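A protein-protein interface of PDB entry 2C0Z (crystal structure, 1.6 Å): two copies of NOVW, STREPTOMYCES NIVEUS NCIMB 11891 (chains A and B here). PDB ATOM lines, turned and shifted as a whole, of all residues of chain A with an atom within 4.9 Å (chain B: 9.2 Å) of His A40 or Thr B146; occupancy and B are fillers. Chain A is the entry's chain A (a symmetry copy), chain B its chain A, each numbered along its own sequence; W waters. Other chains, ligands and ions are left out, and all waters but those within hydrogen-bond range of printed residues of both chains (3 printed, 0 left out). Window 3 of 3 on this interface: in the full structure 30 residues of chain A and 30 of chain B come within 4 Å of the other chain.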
ATOM      1  N   MET A  10      -2.377   6.492  -6.063  1.00  0.00           N
ATOM      2  CA  MET A  10      -2.874   6.976  -7.361  1.00  0.00           C
ATOM      3  C   MET A  10      -1.812   6.830  -8.467  1.00  0.00           C
ATOM      4  O   MET A  10      -0.610   7.013  -8.249  1.00  0.00           O
ATOM      5  CB  MET A  10      -3.320   8.426  -7.205  1.00  0.00           C
ATOM      6  CG  MET A  10      -3.830   9.054  -8.502  1.00  0.00           C
ATOM      7  SD  MET A  10      -4.476  10.695  -8.277  1.00  0.00           S
ATOM      8  CE  MET A  10      -6.032  10.311  -7.593  1.00  0.00           C
ATOM      9  N   TRP A  38     -10.110   9.955  -6.070  1.00  0.00           N
ATOM     10  CA  TRP A  38     -10.205   9.613  -7.490  1.00  0.00           C
ATOM     11  C   TRP A  38      -9.837  10.735  -8.470  1.00  0.00           C
ATOM     12  O   TRP A  38      -9.783  10.489  -9.674  1.00  0.00           O
ATOM     13  CB  TRP A  38     -11.567   9.005  -7.862  1.00  0.00           C
ATOM     14  CG  TRP A  38     -12.775   9.840  -7.681  1.00  0.00           C
ATOM     15  CD1 TRP A  38     -13.367  10.185  -6.511  1.00  0.00           C
ATOM     16  CD2 TRP A  38     -13.583  10.399  -8.709  1.00  0.00           C
ATOM     17  NE1 TRP A  38     -14.508  10.909  -6.748  1.00  0.00           N
ATOM     18  CE2 TRP A  38     -14.657  11.066  -8.096  1.00  0.00           C
ATOM     19  CE3 TRP A  38     -13.518  10.394 -10.102  1.00  0.00           C
ATOM     20  CZ2 TRP A  38     -15.645  11.743  -8.834  1.00  0.00           C
ATOM     21  CZ3 TRP A  38     -14.487  11.066 -10.818  1.00  0.00           C
ATOM     22  CH2 TRP A  38     -15.544  11.712 -10.192  1.00  0.00           C
ATOM     23  N   TYR A  39      -9.607  11.947  -7.944  1.00  0.00           N
ATOM     24  CA  TYR A  39      -9.025  13.052  -8.725  1.00  0.00           C
ATOM     25  C   TYR A  39      -8.163  13.859  -7.779  1.00  0.00           C
ATOM     26  O   TYR A  39      -8.576  14.153  -6.665  1.00  0.00           O
ATOM     27  CB  TYR A  39     -10.114  13.999  -9.290  1.00  0.00           C
ATOM     28  CG  TYR A  39      -9.513  15.205  -9.993  1.00  0.00           C
ATOM     29  CD1 TYR A  39      -9.046  15.104 -11.304  1.00  0.00           C
ATOM     30  CD2 TYR A  39      -9.334  16.407  -9.327  1.00  0.00           C
ATOM     31  CE1 TYR A  39      -8.441  16.204 -11.939  1.00  0.00           C
ATOM     32  CE2 TYR A  39      -8.729  17.471  -9.932  1.00  0.00           C
ATOM     33  CZ  TYR A  39      -8.281  17.361 -11.248  1.00  0.00           C
ATOM     34  OH  TYR A  39      -7.674  18.449 -11.866  1.00  0.00           O
ATOM     35  N   HIS A  40      -6.967  14.206  -8.211  1.00  0.00           N
ATOM     36  CA  HIS A  40      -6.081  15.077  -7.440  1.00  0.00           C
ATOM     37  C   HIS A  40      -5.375  16.046  -8.383  1.00  0.00           C
ATOM     38  O   HIS A  40      -4.709  15.621  -9.316  1.00  0.00           O
ATOM     39  CB  HIS A  40      -5.037  14.251  -6.694  1.00  0.00           C
ATOM     40  CG  HIS A  40      -4.223  15.021  -5.718  1.00  0.00           C
ATOM     41  ND1 HIS A  40      -3.090  15.731  -6.076  1.00  0.00           N
ATOM     42  CD2 HIS A  40      -4.366  15.177  -4.383  1.00  0.00           C
ATOM     43  CE1 HIS A  40      -2.553  16.257  -4.985  1.00  0.00           C
ATOM     44  NE2 HIS A  40      -3.312  15.953  -3.948  1.00  0.00           N
ATOM     45  N   VAL A  41      -5.590  17.336  -8.164  1.00  0.00           N
ATOM     46  CA  VAL A  41      -5.178  18.341  -9.156  1.00  0.00           C
ATOM     47  C   VAL A  41      -3.669  18.330  -9.448  1.00  0.00           C
ATOM     48  O   VAL A  41      -3.262  18.519 -10.595  1.00  0.00           O
ATOM     49  CB  VAL A  41      -5.644  19.745  -8.753  1.00  0.00           C
ATOM     50  CG1 VAL A  41      -4.979  20.209  -7.466  1.00  0.00           C
ATOM     51  CG2 VAL A  41      -5.421  20.737  -9.933  1.00  0.00           C
ATOM     52  N   ASP A  42      -2.844  18.106  -8.432  1.00  0.00           N
ATOM     53  CA  ASP A  42      -1.393  18.156  -8.662  1.00  0.00           C
ATOM     54  C   ASP A  42      -0.949  16.969  -9.505  1.00  0.00           C
ATOM     55  O   ASP A  42      -0.184  17.128 -10.487  1.00  0.00           O
ATOM     56  CB  ASP A  42      -0.622  18.231  -7.355  1.00  0.00           C
ATOM     57  CG  ASP A  42      -1.002  19.420  -6.515  1.00  0.00           C
ATOM     58  OD1 ASP A  42      -1.266  20.511  -7.067  1.00  0.00           O
ATOM     59  OD2 ASP A  42      -1.033  19.335  -5.285  1.00  0.00           O
ATOM     60  N   ARG A  43      -1.472  15.785  -9.171  1.00  0.00           N
ATOM     61  CA  ARG A  43      -1.176  14.588  -9.955  1.00  0.00           C
ATOM     62  C   ARG A  43      -1.678  14.728 -11.391  1.00  0.00           C
ATOM     63  O   ARG A  43      -0.979  14.408 -12.360  1.00  0.00           O
ATOM     64  CB  ARG A  43      -1.773  13.349  -9.313  1.00  0.00           C
ATOM     65  CG  ARG A  43      -1.215  13.083  -7.930  1.00  0.00           C
ATOM     66  CD  ARG A  43       0.263  12.753  -7.858  1.00  0.00           C
ATOM     67  NE  ARG A  43       0.631  11.667  -8.759  1.00  0.00           N
ATOM     68  CZ  ARG A  43       0.497  10.369  -8.479  1.00  0.00           C
ATOM     69  NH1 ARG A  43       0.020   9.969  -7.320  1.00  0.00           N
ATOM     70  NH2 ARG A  43       0.831   9.464  -9.384  1.00  0.00           N
ATOM     71  N   PHE A  44      -2.918  15.162 -11.532  1.00  0.00           N
ATOM     72  CA  PHE A  44      -3.522  15.329 -12.839  1.00  0.00           C
ATOM     73  C   PHE A  44      -2.869  16.393 -13.710  1.00  0.00           C
ATOM     74  O   PHE A  44      -2.571  16.130 -14.872  1.00  0.00           O
ATOM     75  CB  PHE A  44      -5.015  15.656 -12.691  1.00  0.00           C
ATOM     76  CG  PHE A  44      -5.732  15.743 -13.991  1.00  0.00           C
ATOM     77  CD1 PHE A  44      -6.338  14.620 -14.538  1.00  0.00           C
ATOM     78  CD2 PHE A  44      -5.854  16.963 -14.651  1.00  0.00           C
ATOM     79  CE1 PHE A  44      -7.012  14.709 -15.749  1.00  0.00           C
ATOM     80  CE2 PHE A  44      -6.513  17.044 -15.868  1.00  0.00           C
ATOM     81  CZ  PHE A  44      -7.092  15.914 -16.404  1.00  0.00           C
ATOM     82  N   ALA A  45      -2.656  17.580 -13.159  1.00  0.00           N
ATOM     83  CA  ALA A  45      -2.116  18.685 -13.948  1.00  0.00           C
ATOM     84  C   ALA A  45      -0.716  18.346 -14.412  1.00  0.00           C
ATOM     85  O   ALA A  45      -0.339  18.709 -15.526  1.00  0.00           O
ATOM     86  CB  ALA A  45      -2.107  19.974 -13.182  1.00  0.00           C
ATOM     87  N   ARG B  53     -13.587  25.565  -7.301  1.00  0.00           N
ATOM     88  CA  ARG B  53     -12.238  25.156  -7.645  1.00  0.00           C
ATOM     89  C   ARG B  53     -12.114  23.670  -7.351  1.00  0.00           C
ATOM     90  O   ARG B  53     -12.382  23.232  -6.218  1.00  0.00           O
ATOM     91  CB  ARG B  53     -11.247  25.925  -6.755  1.00  0.00           C
ATOM     92  N   LEU B  54     -11.870  22.867  -8.376  1.00  0.00           N
ATOM     93  CA  LEU B  54     -11.720  21.440  -8.163  1.00  0.00           C
ATOM     94  C   LEU B  54     -10.261  21.101  -7.880  1.00  0.00           C
ATOM     95  O   LEU B  54      -9.442  21.074  -8.801  1.00  0.00           O
ATOM     96  CB  LEU B  54     -12.178  20.636  -9.377  1.00  0.00           C
ATOM     97  CG  LEU B  54     -12.031  19.113  -9.254  1.00  0.00           C
ATOM     98  CD1 LEU B  54     -12.957  18.524  -8.210  1.00  0.00           C
ATOM     99  CD2 LEU B  54     -12.225  18.493 -10.647  1.00  0.00           C
ATOM    100  N   ALA B  55      -9.959  20.830  -6.631  1.00  0.00           N
ATOM    101  CA  ALA B  55      -8.639  20.377  -6.240  1.00  0.00           C
ATOM    102  C   ALA B  55      -8.565  18.864  -6.012  1.00  0.00           C
ATOM    103  O   ALA B  55      -7.533  18.223  -6.256  1.00  0.00           O
ATOM    104  CB  ALA B  55      -8.227  21.129  -4.988  1.00  0.00           C
ATOM    105  N   GLN B  56      -9.629  18.284  -5.482  1.00  0.00           N
ATOM    106  CA  GLN B  56      -9.623  16.850  -5.201  1.00  0.00           C
ATOM    107  C   GLN B  56     -11.039  16.317  -5.305  1.00  0.00           C
ATOM    108  O   GLN B  56     -11.988  17.019  -5.039  1.00  0.00           O
ATOM    109  CB  GLN B  56      -9.024  16.591  -3.818  1.00  0.00           C
ATOM    110  CG  GLN B  56      -8.558  15.188  -3.539  1.00  0.00           C
ATOM    111  CD  GLN B  56      -7.738  15.096  -2.233  1.00  0.00           C
ATOM    112  OE1 GLN B  56      -6.718  15.797  -2.046  1.00  0.00           O
ATOM    113  NE2 GLN B  56      -8.153  14.231  -1.366  1.00  0.00           N
ATOM    114  N   ALA B  57     -11.183  15.061  -5.720  1.00  0.00           N
ATOM    115  CA  ALA B  57     -12.478  14.378  -5.698  1.00  0.00           C
ATOM    116  C   ALA B  57     -12.259  13.102  -4.920  1.00  0.00           C
ATOM    117  O   ALA B  57     -11.258  12.406  -5.129  1.00  0.00           O
ATOM    118  CB  ALA B  57     -12.993  14.085  -7.101  1.00  0.00           C
ATOM    119  N   ASN B  58     -13.175  12.805  -4.004  1.00  0.00           N
ATOM    120  CA  ASN B  58     -13.093  11.643  -3.133  1.00  0.00           C
ATOM    121  C   ASN B  58     -14.390  10.864  -3.141  1.00  0.00           C
ATOM    122  O   ASN B  58     -15.451  11.394  -3.501  1.00  0.00           O
ATOM    123  CB  ASN B  58     -12.817  12.059  -1.684  1.00  0.00           C
ATOM    124  CG  ASN B  58     -11.417  12.652  -1.496  1.00  0.00           C
ATOM    125  OD1 ASN B  58     -11.254  13.836  -1.496  1.00  0.00           O
ATOM    126  ND2 ASN B  58     -10.449  11.811  -1.249  1.00  0.00           N
ATOM    127  N   VAL B  73     -11.137  21.967   7.995  1.00  0.00           N
ATOM    128  CA  VAL B  73      -9.800  22.413   7.621  1.00  0.00           C
ATOM    129  C   VAL B  73      -9.546  23.823   8.165  1.00  0.00           C
ATOM    130  O   VAL B  73     -10.393  24.720   8.075  1.00  0.00           O
ATOM    131  CB  VAL B  73      -9.620  22.345   6.080  1.00  0.00           C
ATOM    132  CG1 VAL B  73      -8.307  22.962   5.680  1.00  0.00           C
ATOM    133  CG2 VAL B  73      -9.728  20.888   5.590  1.00  0.00           C
ATOM    134  N   PRO B  77      -5.690  27.767   5.153  1.00  0.00           N
ATOM    135  CA  PRO B  77      -6.177  28.263   3.863  1.00  0.00           C
ATOM    136  C   PRO B  77      -7.692  28.034   3.642  1.00  0.00           C
ATOM    137  O   PRO B  77      -8.301  28.567   2.717  1.00  0.00           O
ATOM    138  CB  PRO B  77      -5.372  27.407   2.873  1.00  0.00           C
ATOM    139  CG  PRO B  77      -5.197  26.122   3.559  1.00  0.00           C
ATOM    140  CD  PRO B  77      -5.115  26.416   5.050  1.00  0.00           C
ATOM    141  N   GLY B  78      -8.268  27.215   4.502  1.00  0.00           N
ATOM    142  CA  GLY B  78      -9.638  26.799   4.379  1.00  0.00           C
ATOM    143  C   GLY B  78      -9.823  25.787   3.271  1.00  0.00           C
ATOM    144  O   GLY B  78      -8.961  25.564   2.424  1.00  0.00           O
ATOM    145  N   GLN B  79     -10.989  25.187   3.281  1.00  0.00           N
ATOM    146  CA  GLN B  79     -11.393  24.239   2.249  1.00  0.00           C
ATOM    147  C   GLN B  79     -12.907  24.294   2.147  1.00  0.00           C
ATOM    148  O   GLN B  79     -13.581  24.332   3.170  1.00  0.00           O
ATOM    149  CB  GLN B  79     -10.993  22.818   2.646  1.00  0.00           C
ATOM    150  CG  GLN B  79     -11.369  21.756   1.610  1.00  0.00           C
ATOM    151  CD  GLN B  79     -11.231  20.364   2.148  1.00  0.00           C
ATOM    152  OE1 GLN B  79     -12.114  19.890   2.870  1.00  0.00           O
ATOM    153  NE2 GLN B  79     -10.130  19.698   1.818  1.00  0.00           N
ATOM    154  N   ALA B  80     -13.415  24.304   0.932  1.00  0.00           N
ATOM    155  CA  ALA B  80     -14.843  24.159   0.688  1.00  0.00           C
ATOM    156  C   ALA B  80     -15.096  22.785   0.096  1.00  0.00           C
ATOM    157  O   ALA B  80     -14.236  22.234  -0.559  1.00  0.00           O
ATOM    158  CB  ALA B  80     -15.293  25.189  -0.271  1.00  0.00           C
ATOM    159  N   LYS B  81     -16.285  22.256   0.343  1.00  0.00           N
ATOM    160  CA  LYS B  81     -16.626  20.895  -0.079  1.00  0.00           C
ATOM    161  C   LYS B  81     -18.013  20.880  -0.694  1.00  0.00           C
ATOM    162  O   LYS B  81     -18.911  21.582  -0.243  1.00  0.00           O
ATOM    163  CB  LYS B  81     -16.645  19.926   1.123  1.00  0.00           C
ATOM    164  CG  LYS B  81     -15.323  19.517   1.660  1.00  0.00           C
ATOM    165  CD  LYS B  81     -15.543  18.420   2.748  1.00  0.00           C
ATOM    166  CE  LYS B  81     -14.544  17.307   2.592  1.00  0.00           C
ATOM    167  NZ  LYS B  81     -13.190  17.827   2.261  1.00  0.00           N
ATOM    168  N   LEU B 142     -16.415  16.757  -3.849  1.00  0.00           N
ATOM    169  CA  LEU B 142     -15.504  17.621  -4.588  1.00  0.00           C
ATOM    170  C   LEU B 142     -14.997  18.693  -3.628  1.00  0.00           C
ATOM    171  O   LEU B 142     -15.804  19.333  -2.928  1.00  0.00           O
ATOM    172  CB  LEU B 142     -16.200  18.253  -5.773  1.00  0.00           C
ATOM    173  CG  LEU B 142     -17.056  17.322  -6.642  1.00  0.00           C
ATOM    174  CD1 LEU B 142     -17.723  18.107  -7.766  1.00  0.00           C
ATOM    175  CD2 LEU B 142     -16.232  16.197  -7.213  1.00  0.00           C
ATOM    176  N   SER B 143     -13.681  18.843  -3.554  1.00  0.00           N
ATOM    177  CA  SER B 143     -13.055  19.747  -2.572  1.00  0.00           C
ATOM    178  C   SER B 143     -12.219  20.789  -3.288  1.00  0.00           C
ATOM    179  O   SER B 143     -11.574  20.492  -4.287  1.00  0.00           O
ATOM    180  CB  SER B 143     -12.159  18.962  -1.602  1.00  0.00           C
ATOM    181  OG  SER B 143     -12.898  18.015  -0.824  1.00  0.00           O
ATOM    182  N   SER B 144     -12.197  21.997  -2.718  1.00  0.00           N
ATOM    183  CA  SER B 144     -11.418  23.108  -3.256  1.00  0.00           C
ATOM    184  C   SER B 144      -9.948  23.107  -2.859  1.00  0.00           C
ATOM    185  O   SER B 144      -9.200  23.948  -3.323  1.00  0.00           O
ATOM    186  CB  SER B 144     -12.044  24.436  -2.829  1.00  0.00           C
ATOM    187  OG  SER B 144     -11.824  24.665  -1.426  1.00  0.00           O
ATOM    188  N   GLY B 145      -9.532  22.219  -1.978  1.00  0.00           N
ATOM    189  CA  GLY B 145      -8.124  22.060  -1.642  1.00  0.00           C
ATOM    190  C   GLY B 145      -7.751  20.612  -1.498  1.00  0.00           C
ATOM    191  O   GLY B 145      -8.604  19.746  -1.253  1.00  0.00           O
ATOM    192  N   THR B 146      -6.468  20.331  -1.656  1.00  0.00           N
ATOM    193  CA  THR B 146      -6.001  18.963  -1.509  1.00  0.00           C
ATOM    194  C   THR B 146      -5.747  18.634  -0.053  1.00  0.00           C
ATOM    195  O   THR B 146      -5.573  19.529   0.801  1.00  0.00           O
ATOM    196  CB  THR B 146      -4.713  18.728  -2.295  1.00  0.00           C
ATOM    197  OG1 THR B 146      -3.722  19.697  -1.930  1.00  0.00           O
ATOM    198  CG2 THR B 146      -4.949  18.884  -3.793  1.00  0.00           C
ATOM    199  N   TYR B 147      -5.765  17.346   0.242  1.00  0.00           N
ATOM    200  CA  TYR B 147      -5.515  16.881   1.599  1.00  0.00           C
ATOM    201  C   TYR B 147      -4.146  17.309   2.080  1.00  0.00           C
ATOM    202  O   TYR B 147      -3.125  17.121   1.406  1.00  0.00           O
ATOM    203  CB  TYR B 147      -5.624  15.362   1.661  1.00  0.00           C
ATOM    204  CG  TYR B 147      -5.258  14.789   3.014  1.00  0.00           C
ATOM    205  CD1 TYR B 147      -6.076  14.998   4.112  1.00  0.00           C
ATOM    206  CD2 TYR B 147      -4.096  14.049   3.183  1.00  0.00           C
ATOM    207  CE1 TYR B 147      -5.753  14.482   5.360  1.00  0.00           C
ATOM    208  CE2 TYR B 147      -3.754  13.521   4.434  1.00  0.00           C
ATOM    209  CZ  TYR B 147      -4.593  13.746   5.509  1.00  0.00           C
ATOM    210  OH  TYR B 147      -4.277  13.228   6.742  1.00  0.00           O
ATOM    211  N   ASP B 148      -4.144  17.902   3.266  1.00  0.00           N
ATOM    212  CA  ASP B 148      -2.937  18.270   3.975  1.00  0.00           C
ATOM    213  C   ASP B 148      -3.146  17.842   5.435  1.00  0.00           C
ATOM    214  O   ASP B 148      -4.049  18.352   6.118  1.00  0.00           O
ATOM    215  CB  ASP B 148      -2.735  19.768   3.848  1.00  0.00           C
ATOM    216  CG  ASP B 148      -1.484  20.256   4.538  1.00  0.00           C
ATOM    217  OD1 ASP B 148      -0.851  19.459   5.257  1.00  0.00           O
ATOM    218  OD2 ASP B 148      -1.094  21.435   4.432  1.00  0.00           O
ATOM    219  N   PRO B 149      -2.353  16.892   5.934  1.00  0.00           N
ATOM    220  CA  PRO B 149      -2.575  16.393   7.306  1.00  0.00           C
ATOM    221  C   PRO B 149      -2.374  17.473   8.377  1.00  0.00           C
ATOM    222  O   PRO B 149      -2.929  17.378   9.462  1.00  0.00           O
ATOM    223  CB  PRO B 149      -1.533  15.264   7.447  1.00  0.00           C
ATOM    224  CG  PRO B 149      -0.478  15.582   6.432  1.00  0.00           C
ATOM    225  CD  PRO B 149      -1.199  16.245   5.282  1.00  0.00           C
ATOM    226  N   ALA B 150      -1.632  18.519   8.058  1.00  0.00           N
ATOM    227  CA  ALA B 150      -1.362  19.604   8.992  1.00  0.00           C
ATOM    228  C   ALA B 150      -2.565  20.503   9.249  1.00  0.00           C
ATOM    229  O   ALA B 150      -2.613  21.213  10.267  1.00  0.00           O
ATOM    230  CB  ALA B 150      -0.208  20.459   8.475  1.00  0.00           C
ATOM    231  N   THR B 151      -3.520  20.512   8.317  1.00  0.00           N
ATOM    232  CA  THR B 151      -4.645  21.443   8.412  1.00  0.00           C
ATOM    233  C   THR B 151      -5.982  20.769   8.647  1.00  0.00           C
ATOM    234  O   THR B 151      -6.961  21.478   8.879  1.00  0.00           O
ATOM    235  CB  THR B 151      -4.763  22.326   7.160  1.00  0.00           C
ATOM    236  OG1 THR B 151      -4.987  21.512   6.000  1.00  0.00           O
ATOM    237  CG2 THR B 151      -3.473  23.056   6.894  1.00  0.00           C
ATOM    238  N   GLU B 152      -6.049  19.445   8.559  1.00  0.00           N
ATOM    239  CA  GLU B 152      -7.329  18.761   8.776  1.00  0.00           C
ATOM    240  C   GLU B 152      -7.508  18.344  10.218  1.00  0.00           C
ATOM    241  O   GLU B 152      -6.702  17.581  10.776  1.00  0.00           O
ATOM    242  CB  GLU B 152      -7.536  17.540   7.887  1.00  0.00           C
ATOM    243  CG  GLU B 152      -9.007  17.107   7.945  1.00  0.00           C
ATOM    244  CD  GLU B 152      -9.322  15.946   7.035  1.00  0.00           C
ATOM    245  OE1 GLU B 152      -8.918  16.000   5.861  1.00  0.00           O
ATOM    246  OE2 GLU B 152      -9.986  14.989   7.494  1.00  0.00           O
HETATM  247  O   HOH W   1      -2.191  21.236  -3.863  1.00  0.00           O
HETATM  248  O   HOH W   2      -8.710  20.789 -11.275  1.00  0.00           O
HETATM  249  O   HOH W   3      -2.809  15.827  -1.031  1.00  0.00           O
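Of the printed residues of chain B, Trp A38 touches Ala B57 and Asn B58. His A40 touches just these residues of chain B: Ala B55, Gln B56 and Thr B146. No residue of chain B comes within 4 Å of Asp A42. Printed residues of chain A within 4 Å of Leu B54: Tyr A39. Printed residues of chain A within 4 Å of Ala B55: Tyr A39 (3.9 Å), His A40 (3.7 Å) and Val A41 (2.9 Å). Printed residues of chain A within 4 Å of Gln B56: Tyr A39 and His A40. Of chain A, only His A40 and Val A41 come within 4 Å of Thr B146. The nearest residue of chain B that does not touch His A40 is Ala B57 (5.0 Å). The nearest printed residue of chain A that does not touch Ala B55 is Asp A42 (5.2 Å).
Of the 9 printed residues of chain A, 4 touch a printed residue of chain B. Hydrophobic or aromatic side chains of chain A that line the printed part of chain B: Trp A38, Tyr A39, His A40 and Val A41. Of the 23 printed residues of chain B, 6 touch a printed residue of chain A. Hydrophobic or aromatic side chains of chain B that line the printed part of chain A: Leu B54 and Ala B57. Among the printed residues, no Asp or Glu carboxylate lies within 4 Å of a Lys or Arg side-chain nitrogen of the other chain.
The backbone carbonyl oxygen of Ala B55 lies within hydrogen-bond range of the backbone NH of Val A41, 2.9 Å away. O of Ala B57 sits at hydrogen-bond distance from N of Trp A38. The backbone NH of Ala B57 is in hydrogen-bond range of the backbone carbonyl oxygen of Tyr A39, 2.9 Å away. The indole nitrogen (NE1) of Trp A38 sits at hydrogen-bond distance from the backbone carbonyl oxygen (O) of Asn B58 (3.4 Å).
No position is printed for both chains. Of the 11 pairs that touch across the chains among the printed residues, none has its exchanged pair printed and touching as well.
Tyr A39 touches Leu B54. Tyr A39 touches Ala B55 (CE2 to O, 3.9 Å). CA of Gln B56 touches O of Tyr A39, at 3.2 Å. Ala B55 touches His A40 (O to CA, 3.7 Å). His A40 touches Gln B56 (CD2 to OE1, 3.4 Å). Thr B146 touches His A40. Thr B146 touches Val A41.
The backbone NH (N) of Ala B55 sits at hydrogen-bond distance from the backbone carbonyl oxygen (O) of Ser B143, 2.9 Å away. The side-chain amide oxygen of Asn B58 sits at hydrogen-bond distance from the side-chain amide nitrogen of Gln B56, at 3.1 Å. N of Ser B143 lies within hydrogen-bond range of O of Gln B56 (2.9 Å). N of Tyr B147 lies within hydrogen-bond range of OE1 of Gln B56 (2.9 Å). A ring nitrogen (ND1) of His A40 lies close to the backbone NH (N) of Asp A42, at 3.4 Å. A ring nitrogen (ND1) of His A40 is in hydrogen-bond range of the backbone NH (N) of Arg A43 (3.5 Å).
Water W2 bridges O of Leu B54 (2.6 Å) and OH of Tyr A39 (2.6 Å). Water W1 bridges OD2 of Asp A42 (2.6 Å) and OG1 of Thr B146 (2.9 Å). Water W3 bridges the backbone carbonyl oxygen (O) of Tyr B147 (2.8 Å) and a ring nitrogen (NE2) of His A40 (3.0 Å).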
